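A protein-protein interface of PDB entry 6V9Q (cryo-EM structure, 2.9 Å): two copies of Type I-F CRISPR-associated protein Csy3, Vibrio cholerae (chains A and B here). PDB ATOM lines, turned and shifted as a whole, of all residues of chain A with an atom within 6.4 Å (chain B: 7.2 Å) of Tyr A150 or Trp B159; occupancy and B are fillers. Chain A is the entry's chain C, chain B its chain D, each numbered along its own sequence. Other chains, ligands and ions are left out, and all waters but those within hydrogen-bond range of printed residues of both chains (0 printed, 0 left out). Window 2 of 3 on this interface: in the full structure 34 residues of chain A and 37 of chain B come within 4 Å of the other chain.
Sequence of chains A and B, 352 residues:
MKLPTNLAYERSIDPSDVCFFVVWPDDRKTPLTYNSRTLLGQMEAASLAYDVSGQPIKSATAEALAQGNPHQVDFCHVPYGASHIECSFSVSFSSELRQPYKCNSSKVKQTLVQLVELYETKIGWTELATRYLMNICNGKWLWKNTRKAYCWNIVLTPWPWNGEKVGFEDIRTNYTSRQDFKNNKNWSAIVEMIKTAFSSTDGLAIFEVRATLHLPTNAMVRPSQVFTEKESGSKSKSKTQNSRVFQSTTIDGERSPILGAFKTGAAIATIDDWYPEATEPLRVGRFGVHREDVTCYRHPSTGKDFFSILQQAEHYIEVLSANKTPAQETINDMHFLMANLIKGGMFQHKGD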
ATOM      1  N   THR A 146      18.947   9.954  20.924  1.00  0.00           N
ATOM      2  CA  THR A 146      18.872   8.571  21.371  1.00  0.00           C
ATOM      3  C   THR A 146      18.415   7.653  20.250  1.00  0.00           C
ATOM      4  O   THR A 146      18.993   6.581  20.037  1.00  0.00           O
ATOM      5  CB  THR A 146      17.924   8.522  22.570  1.00  0.00           C
ATOM      6  OG1 THR A 146      18.587   9.001  23.743  1.00  0.00           O
ATOM      7  CG2 THR A 146      17.314   7.176  22.791  1.00  0.00           C
ATOM      8  N   LYS A 148      18.119   6.210  16.586  1.00  0.00           N
ATOM      9  CA  LYS A 148      19.108   5.987  15.518  1.00  0.00           C
ATOM     10  C   LYS A 148      20.546   6.053  16.028  1.00  0.00           C
ATOM     11  O   LYS A 148      21.422   6.609  15.370  1.00  0.00           O
ATOM     12  CB  LYS A 148      18.932   6.956  14.347  1.00  0.00           C
ATOM     13  CG  LYS A 148      17.609   6.913  13.652  1.00  0.00           C
ATOM     14  CD  LYS A 148      17.601   8.002  12.623  1.00  0.00           C
ATOM     15  CE  LYS A 148      16.329   8.022  11.830  1.00  0.00           C
ATOM     16  NZ  LYS A 148      15.179   8.383  12.694  1.00  0.00           N
ATOM     17  N   ALA A 149      20.807   5.466  17.190  1.00  0.00           N
ATOM     18  CA  ALA A 149      22.149   5.429  17.749  1.00  0.00           C
ATOM     19  C   ALA A 149      22.574   3.993  18.017  1.00  0.00           C
ATOM     20  O   ALA A 149      21.748   3.085  18.120  1.00  0.00           O
ATOM     21  CB  ALA A 149      22.236   6.239  19.043  1.00  0.00           C
ATOM     22  N   TYR A 150      23.885   3.793  18.129  1.00  0.00           N
ATOM     23  CA  TYR A 150      24.404   2.478  18.488  1.00  0.00           C
ATOM     24  C   TYR A 150      24.181   2.191  19.967  1.00  0.00           C
ATOM     25  O   TYR A 150      23.499   1.227  20.328  1.00  0.00           O
ATOM     26  CB  TYR A 150      25.886   2.392  18.139  1.00  0.00           C
ATOM     27  CG  TYR A 150      26.181   2.306  16.669  1.00  0.00           C
ATOM     28  CD1 TYR A 150      25.282   1.739  15.794  1.00  0.00           C
ATOM     29  CD2 TYR A 150      27.340   2.849  16.151  1.00  0.00           C
ATOM     30  CE1 TYR A 150      25.553   1.668  14.453  1.00  0.00           C
ATOM     31  CE2 TYR A 150      27.610   2.795  14.811  1.00  0.00           C
ATOM     32  CZ  TYR A 150      26.713   2.202  13.968  1.00  0.00           C
ATOM     33  OH  TYR A 150      26.975   2.141  12.627  1.00  0.00           O
ATOM     34  N   CYS A 151      24.749   3.019  20.839  1.00  0.00           N
ATOM     35  CA  CYS A 151      24.529   2.891  22.271  1.00  0.00           C
ATOM     36  C   CYS A 151      24.755   4.242  22.927  1.00  0.00           C
ATOM     37  O   CYS A 151      25.406   5.121  22.364  1.00  0.00           O
ATOM     38  CB  CYS A 151      25.448   1.838  22.897  1.00  0.00           C
ATOM     39  SG  CYS A 151      27.190   2.243  22.855  1.00  0.00           S
ATOM     40  N   TRP A 152      24.200   4.403  24.127  1.00  0.00           N
ATOM     41  CA  TRP A 152      24.427   5.605  24.911  1.00  0.00           C
ATOM     42  C   TRP A 152      24.551   5.231  26.382  1.00  0.00           C
ATOM     43  O   TRP A 152      23.934   4.275  26.849  1.00  0.00           O
ATOM     44  CB  TRP A 152      23.332   6.659  24.668  1.00  0.00           C
ATOM     45  CG  TRP A 152      21.960   6.280  25.086  1.00  0.00           C
ATOM     46  CD1 TRP A 152      21.341   6.613  26.246  1.00  0.00           C
ATOM     47  CD2 TRP A 152      21.036   5.476  24.356  1.00  0.00           C
ATOM     48  NE1 TRP A 152      20.083   6.077  26.281  1.00  0.00           N
ATOM     49  CE2 TRP A 152      19.875   5.369  25.130  1.00  0.00           C
ATOM     50  CE3 TRP A 152      21.081   4.835  23.119  1.00  0.00           C
ATOM     51  CZ2 TRP A 152      18.778   4.641  24.717  1.00  0.00           C
ATOM     52  CZ3 TRP A 152      19.993   4.128  22.709  1.00  0.00           C
ATOM     53  CH2 TRP A 152      18.852   4.036  23.499  1.00  0.00           C
ATOM     54  N   ASP A 170      25.151   1.023  28.395  1.00  0.00           N
ATOM     55  CA  ASP A 170      24.445   0.351  27.303  1.00  0.00           C
ATOM     56  C   ASP A 170      22.944   0.255  27.579  1.00  0.00           C
ATOM     57  O   ASP A 170      22.367  -0.824  27.696  1.00  0.00           O
ATOM     58  CB  ASP A 170      25.050  -1.031  27.025  1.00  0.00           C
ATOM     59  CG  ASP A 170      24.652  -1.589  25.670  1.00  0.00           C
ATOM     60  OD1 ASP A 170      23.950  -0.894  24.907  1.00  0.00           O
ATOM     61  OD2 ASP A 170      25.043  -2.737  25.372  1.00  0.00           O
ATOM     62  N   ILE A 171      22.319   1.426  27.674  1.00  0.00           N
ATOM     63  CA  ILE A 171      20.875   1.503  27.607  1.00  0.00           C
ATOM     64  C   ILE A 171      20.456   1.114  26.187  1.00  0.00           C
ATOM     65  O   ILE A 171      21.245   1.215  25.238  1.00  0.00           O
ATOM     66  CB  ILE A 171      20.447   2.932  27.970  1.00  0.00           C
ATOM     67  CG1 ILE A 171      21.198   3.363  29.212  1.00  0.00           C
ATOM     68  CG2 ILE A 171      18.988   3.018  28.341  1.00  0.00           C
ATOM     69  CD1 ILE A 171      21.115   4.797  29.456  1.00  0.00           C
ATOM     70  N   ARG A 172      19.188   0.693  26.048  1.00  0.00           N
ATOM     71  CA  ARG A 172      18.501  -0.075  25.003  1.00  0.00           C
ATOM     72  C   ARG A 172      18.828  -1.569  25.146  1.00  0.00           C
ATOM     73  O   ARG A 172      18.140  -2.397  24.552  1.00  0.00           O
ATOM     74  CB  ARG A 172      18.807   0.401  23.558  1.00  0.00           C
ATOM     75  CG  ARG A 172      17.934  -0.099  22.407  1.00  0.00           C
ATOM     76  CD  ARG A 172      18.489   0.302  21.035  1.00  0.00           C
ATOM     77  NE  ARG A 172      18.351   1.720  20.718  1.00  0.00           N
ATOM     78  CZ  ARG A 172      17.270   2.246  20.148  1.00  0.00           C
ATOM     79  NH1 ARG A 172      16.243   1.464  19.839  1.00  0.00           N
ATOM     80  NH2 ARG A 172      17.210   3.545  19.887  1.00  0.00           N
ATOM     81  N   HIS A 214      27.191   7.107  20.842  1.00  0.00           N
ATOM     82  CA  HIS A 214      27.901   6.510  19.719  1.00  0.00           C
ATOM     83  C   HIS A 214      26.952   6.497  18.529  1.00  0.00           C
ATOM     84  O   HIS A 214      26.084   5.632  18.423  1.00  0.00           O
ATOM     85  CB  HIS A 214      28.390   5.117  20.085  1.00  0.00           C
ATOM     86  CG  HIS A 214      29.423   5.119  21.165  1.00  0.00           C
ATOM     87  ND1 HIS A 214      30.756   5.353  20.917  1.00  0.00           N
ATOM     88  CD2 HIS A 214      29.311   4.976  22.506  1.00  0.00           C
ATOM     89  CE1 HIS A 214      31.426   5.318  22.054  1.00  0.00           C
ATOM     90  NE2 HIS A 214      30.572   5.094  23.033  1.00  0.00           N
ATOM     91  N   LEU A 215      27.102   7.471  17.648  1.00  0.00           N
ATOM     92  CA  LEU A 215      26.271   7.608  16.462  1.00  0.00           C
ATOM     93  C   LEU A 215      26.901   6.855  15.303  1.00  0.00           C
ATOM     94  O   LEU A 215      28.048   6.423  15.384  1.00  0.00           O
ATOM     95  CB  LEU A 215      26.102   9.090  16.119  1.00  0.00           C
ATOM     96  CG  LEU A 215      24.973   9.925  16.717  1.00  0.00           C
ATOM     97  CD1 LEU A 215      23.642   9.282  16.449  1.00  0.00           C
ATOM     98  CD2 LEU A 215      25.152  10.146  18.162  1.00  0.00           C
ATOM     99  N   PRO A 216      26.172   6.672  14.180  1.00  0.00           N
ATOM    100  CA  PRO A 216      26.829   6.186  12.960  1.00  0.00           C
ATOM    101  C   PRO A 216      27.795   7.182  12.339  1.00  0.00           C
ATOM    102  O   PRO A 216      28.040   8.258  12.890  1.00  0.00           O
ATOM    103  CB  PRO A 216      25.652   5.917  12.020  1.00  0.00           C
ATOM    104  CG  PRO A 216      24.540   5.680  12.890  1.00  0.00           C
ATOM    105  CD  PRO A 216      24.709   6.545  14.066  1.00  0.00           C
ATOM    106  N   THR A 217      28.359   6.821  11.193  1.00  0.00           N
ATOM    107  CA  THR A 217      29.295   7.694  10.494  1.00  0.00           C
ATOM    108  C   THR A 217      28.579   8.929   9.988  1.00  0.00           C
ATOM    109  O   THR A 217      27.544   8.817   9.326  1.00  0.00           O
ATOM    110  CB  THR A 217      29.944   6.958   9.329  1.00  0.00           C
ATOM    111  OG1 THR A 217      30.766   5.899   9.830  1.00  0.00           O
ATOM    112  CG2 THR A 217      30.778   7.899   8.490  1.00  0.00           C
ATOM    113  N   SER B  90      26.176   6.761   5.646  1.00  0.00           N
ATOM    114  CA  SER B  90      25.384   5.834   6.442  1.00  0.00           C
ATOM    115  C   SER B  90      23.897   6.132   6.310  1.00  0.00           C
ATOM    116  O   SER B  90      23.494   7.286   6.182  1.00  0.00           O
ATOM    117  CB  SER B  90      25.771   5.902   7.911  1.00  0.00           C
ATOM    118  OG  SER B  90      25.421   7.162   8.439  1.00  0.00           O
ATOM    119  N   THR B 157      27.919  -2.595   5.737  1.00  0.00           N
ATOM    120  CA  THR B 157      28.191  -3.027   7.107  1.00  0.00           C
ATOM    121  C   THR B 157      26.949  -2.768   7.946  1.00  0.00           C
ATOM    122  O   THR B 157      26.794  -1.695   8.541  1.00  0.00           O
ATOM    123  CB  THR B 157      29.408  -2.311   7.689  1.00  0.00           C
ATOM    124  OG1 THR B 157      30.507  -2.459   6.790  1.00  0.00           O
ATOM    125  CG2 THR B 157      29.802  -2.919   9.014  1.00  0.00           C
ATOM    126  N   PRO B 158      26.028  -3.725   7.999  1.00  0.00           N
ATOM    127  CA  PRO B 158      24.792  -3.529   8.758  1.00  0.00           C
ATOM    128  C   PRO B 158      25.008  -3.687  10.253  1.00  0.00           C
ATOM    129  O   PRO B 158      25.885  -4.427  10.700  1.00  0.00           O
ATOM    130  CB  PRO B 158      23.877  -4.621   8.203  1.00  0.00           C
ATOM    131  CG  PRO B 158      24.782  -5.630   7.678  1.00  0.00           C
ATOM    132  CD  PRO B 158      25.980  -4.948   7.185  1.00  0.00           C
ATOM    133  N   TRP B 159      24.241  -2.923  11.039  1.00  0.00           N
ATOM    134  CA  TRP B 159      24.595  -2.967  12.452  1.00  0.00           C
ATOM    135  C   TRP B 159      23.980  -4.126  13.233  1.00  0.00           C
ATOM    136  O   TRP B 159      24.745  -4.861  13.871  1.00  0.00           O
ATOM    137  CB  TRP B 159      24.309  -1.657  13.180  1.00  0.00           C
ATOM    138  CG  TRP B 159      24.629  -1.824  14.620  1.00  0.00           C
ATOM    139  CD1 TRP B 159      25.832  -2.174  15.153  1.00  0.00           C
ATOM    140  CD2 TRP B 159      23.734  -1.676  15.713  1.00  0.00           C
ATOM    141  NE1 TRP B 159      25.741  -2.252  16.514  1.00  0.00           N
ATOM    142  CE2 TRP B 159      24.460  -1.945  16.884  1.00  0.00           C
ATOM    143  CE3 TRP B 159      22.390  -1.329  15.817  1.00  0.00           C
ATOM    144  CZ2 TRP B 159      23.886  -1.876  18.139  1.00  0.00           C
ATOM    145  CZ3 TRP B 159      21.824  -1.266  17.056  1.00  0.00           C
ATOM    146  CH2 TRP B 159      22.567  -1.537  18.205  1.00  0.00           C
ATOM    147  N   PRO B 160      22.635  -4.355  13.257  1.00  0.00           N
ATOM    148  CA  PRO B 160      22.239  -5.512  14.098  1.00  0.00           C
ATOM    149  C   PRO B 160      22.467  -6.835  13.367  1.00  0.00           C
ATOM    150  O   PRO B 160      21.559  -7.535  12.937  1.00  0.00           O
ATOM    151  CB  PRO B 160      20.766  -5.226  14.388  1.00  0.00           C
ATOM    152  CG  PRO B 160      20.304  -4.489  13.209  1.00  0.00           C
ATOM    153  CD  PRO B 160      21.448  -3.665  12.712  1.00  0.00           C
ATOM    154  N   TRP B 161      23.741  -7.212  13.279  1.00  0.00           N
ATOM    155  CA  TRP B 161      24.233  -8.174  12.310  1.00  0.00           C
ATOM    156  C   TRP B 161      25.347  -8.991  12.940  1.00  0.00           C
ATOM    157  O   TRP B 161      26.112  -8.484  13.761  1.00  0.00           O
ATOM    158  CB  TRP B 161      24.735  -7.438  11.069  1.00  0.00           C
ATOM    159  CG  TRP B 161      25.327  -8.252   9.981  1.00  0.00           C
ATOM    160  CD1 TRP B 161      26.648  -8.448   9.748  1.00  0.00           C
ATOM    161  CD2 TRP B 161      24.632  -8.909   8.921  1.00  0.00           C
ATOM    162  NE1 TRP B 161      26.821  -9.214   8.630  1.00  0.00           N
ATOM    163  CE2 TRP B 161      25.596  -9.508   8.105  1.00  0.00           C
ATOM    164  CE3 TRP B 161      23.287  -9.059   8.594  1.00  0.00           C
ATOM    165  CZ2 TRP B 161      25.264 -10.249   6.986  1.00  0.00           C
ATOM    166  CZ3 TRP B 161      22.957  -9.790   7.484  1.00  0.00           C
ATOM    167  CH2 TRP B 161      23.940 -10.384   6.700  1.00  0.00           C
ATOM    168  N   ASN B 162      25.439 -10.258  12.536  1.00  0.00           N
ATOM    169  CA  ASN B 162      26.428 -11.176  13.086  1.00  0.00           C
ATOM    170  C   ASN B 162      27.842 -10.846  12.625  1.00  0.00           C
ATOM    171  O   ASN B 162      28.689 -10.465  13.437  1.00  0.00           O
ATOM    172  CB  ASN B 162      26.083 -12.616  12.707  1.00  0.00           C
ATOM    173  CG  ASN B 162      24.911 -13.164  13.501  1.00  0.00           C
ATOM    174  OD1 ASN B 162      24.780 -12.901  14.698  1.00  0.00           O
ATOM    175  ND2 ASN B 162      24.071 -13.955  12.848  1.00  0.00           N
ATOM    176  N   MET B 193      16.031  -7.036   7.251  1.00  0.00           N
ATOM    177  CA  MET B 193      16.262  -5.990   8.240  1.00  0.00           C
ATOM    178  C   MET B 193      15.344  -4.808   8.012  1.00  0.00           C
ATOM    179  O   MET B 193      14.780  -4.263   8.962  1.00  0.00           O
ATOM    180  CB  MET B 193      17.700  -5.497   8.198  1.00  0.00           C
ATOM    181  CG  MET B 193      18.688  -6.351   8.889  1.00  0.00           C
ATOM    182  SD  MET B 193      20.218  -5.445   8.853  1.00  0.00           S
ATOM    183  CE  MET B 193      21.191  -6.496   9.904  1.00  0.00           C
ATOM    184  N   LEU B 204      15.245  -0.365  13.840  1.00  0.00           N
ATOM    185  CA  LEU B 204      16.417   0.498  13.851  1.00  0.00           C
ATOM    186  C   LEU B 204      17.252   0.432  12.575  1.00  0.00           C
ATOM    187  O   LEU B 204      17.436   1.478  11.950  1.00  0.00           O
ATOM    188  CB  LEU B 204      17.211   0.166  15.119  1.00  0.00           C
ATOM    189  CG  LEU B 204      18.273   1.109  15.665  1.00  0.00           C
ATOM    190  CD1 LEU B 204      19.592   0.777  15.087  1.00  0.00           C
ATOM    191  CD2 LEU B 204      17.915   2.513  15.312  1.00  0.00           C
ATOM    192  N   ALA B 205      17.793  -0.736  12.195  1.00  0.00           N
ATOM    193  CA  ALA B 205      18.455  -1.012  10.909  1.00  0.00           C
ATOM    194  C   ALA B 205      19.455   0.010  10.360  1.00  0.00           C
ATOM    195  O   ALA B 205      19.120   0.741   9.430  1.00  0.00           O
ATOM    196  CB  ALA B 205      17.399  -1.245   9.838  1.00  0.00           C
ATOM    197  N   ILE B 206      20.656   0.106  10.924  1.00  0.00           N
ATOM    198  CA  ILE B 206      21.683   1.030  10.445  1.00  0.00           C
ATOM    199  C   ILE B 206      22.605   0.319   9.459  1.00  0.00           C
ATOM    200  O   ILE B 206      23.056  -0.800   9.720  1.00  0.00           O
ATOM    201  CB  ILE B 206      22.482   1.614  11.621  1.00  0.00           C
ATOM    202  CG1 ILE B 206      21.580   2.461  12.499  1.00  0.00           C
ATOM    203  CG2 ILE B 206      23.605   2.489  11.148  1.00  0.00           C
ATOM    204  CD1 ILE B 206      22.242   2.902  13.760  1.00  0.00           C
ATOM    205  N   PHE B 207      22.887   0.968   8.329  1.00  0.00           N
ATOM    206  CA  PHE B 207      23.867   0.515   7.351  1.00  0.00           C
ATOM    207  C   PHE B 207      25.037   1.485   7.292  1.00  0.00           C
ATOM    208  O   PHE B 207      24.843   2.699   7.278  1.00  0.00           O
ATOM    209  CB  PHE B 207      23.236   0.417   5.968  1.00  0.00           C
ATOM    210  CG  PHE B 207      22.210  -0.652   5.849  1.00  0.00           C
ATOM    211  CD1 PHE B 207      22.283  -1.789   6.615  1.00  0.00           C
ATOM    212  CD2 PHE B 207      21.124  -0.484   5.027  1.00  0.00           C
ATOM    213  CE1 PHE B 207      21.320  -2.763   6.517  1.00  0.00           C
ATOM    214  CE2 PHE B 207      20.157  -1.459   4.937  1.00  0.00           C
ATOM    215  CZ  PHE B 207      20.261  -2.592   5.688  1.00  0.00           C
ATOM    216  N   GLU B 208      26.250   0.946   7.257  1.00  0.00           N
ATOM    217  CA  GLU B 208      27.467   1.694   6.960  1.00  0.00           C
ATOM    218  C   GLU B 208      27.858   1.321   5.539  1.00  0.00           C
ATOM    219  O   GLU B 208      28.185   0.163   5.274  1.00  0.00           O
ATOM    220  CB  GLU B 208      28.592   1.331   7.922  1.00  0.00           C
ATOM    221  CG  GLU B 208      28.396   1.680   9.381  1.00  0.00           C
ATOM    222  CD  GLU B 208      28.659   3.127   9.682  1.00  0.00           C
ATOM    223  OE1 GLU B 208      29.483   3.726   8.974  1.00  0.00           O
ATOM    224  OE2 GLU B 208      28.074   3.654  10.647  1.00  0.00           O
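Of chain B, only Trp B159 (3.6 Å), Ile B206 (3.6 Å) and Glu B208 (2.7 Å) come within 4 Å of Tyr A150.
Trp B159 touches just one residue of chain A: Tyr A150.
Printed residues of chain A within 4 Å of Leu B204: Lys A148 (3.7 Å).
Of the printed residues of chain B, Thr A217 touches Ser B90 and Glu B208.
Printed residues of chain A within 4 Å of Ser B90: Pro A216 (3.8 Å) and Thr A217 (2.8 Å).
The nearest residue of chain B that does not touch Tyr A150 is Thr B157 (5.6 Å).
The nearest residue of chain A that does not touch Trp B159 is Ala A149 (4.5 Å).
The nearest printed residue of chain B that does not touch Lys A148 is Ile B206 (4.1 Å).
No position is printed for both chains.
Of the 9 pairs that touch across the chains among the printed residues, none has its exchanged pair printed and touching as well.
The side-chain hydroxyl of Tyr A150 sits at hydrogen-bond distance from the side-chain carboxylate of Glu B208 (2.7 Å).
OG1 of Thr A217 is in hydrogen-bond range of OE1 of Glu B208 (2.7 Å).
O of Thr A217 sits at hydrogen-bond distance from OG of Ser B90 (2.8 Å).
Of the 13 printed residues of chain B, 5 touch a printed residue of chain A.
Hydrophobic or aromatic side chains of chain B within 4 Å of the printed part of chain A: Trp B159, Leu B204 and Ile B206.
Printed residues of chain A that touch a printed residue of chain B: Lys A148, Tyr A150, Pro A216 and Thr A217.
Along chain A the printed residues that touch a printed residue of chain B span positions 148 to 217.
Lys A148 touches Leu B204.
Tyr A150 touches Trp B159.
Tyr A150 touches Ile B206 (CE1 to CD1, 3.6 Å).
OG of Ser B90 touches CB of Pro A216, at 3.8 Å.
Ile B206 touches Pro A216.
Pro A216 touches Glu B208.
The backbone carbonyl oxygen (O) of His A214 is in hydrogen-bond range of the backbone NH (N) of Tyr A150, at 2.9 Å.
The backbone NH (N) of Trp B159 lies within hydrogen-bond range of the backbone carbonyl oxygen (O) of Ile B206 (2.8 Å).
N of Thr B157 lies within hydrogen-bond range of O of Glu B208 (2.8 Å).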
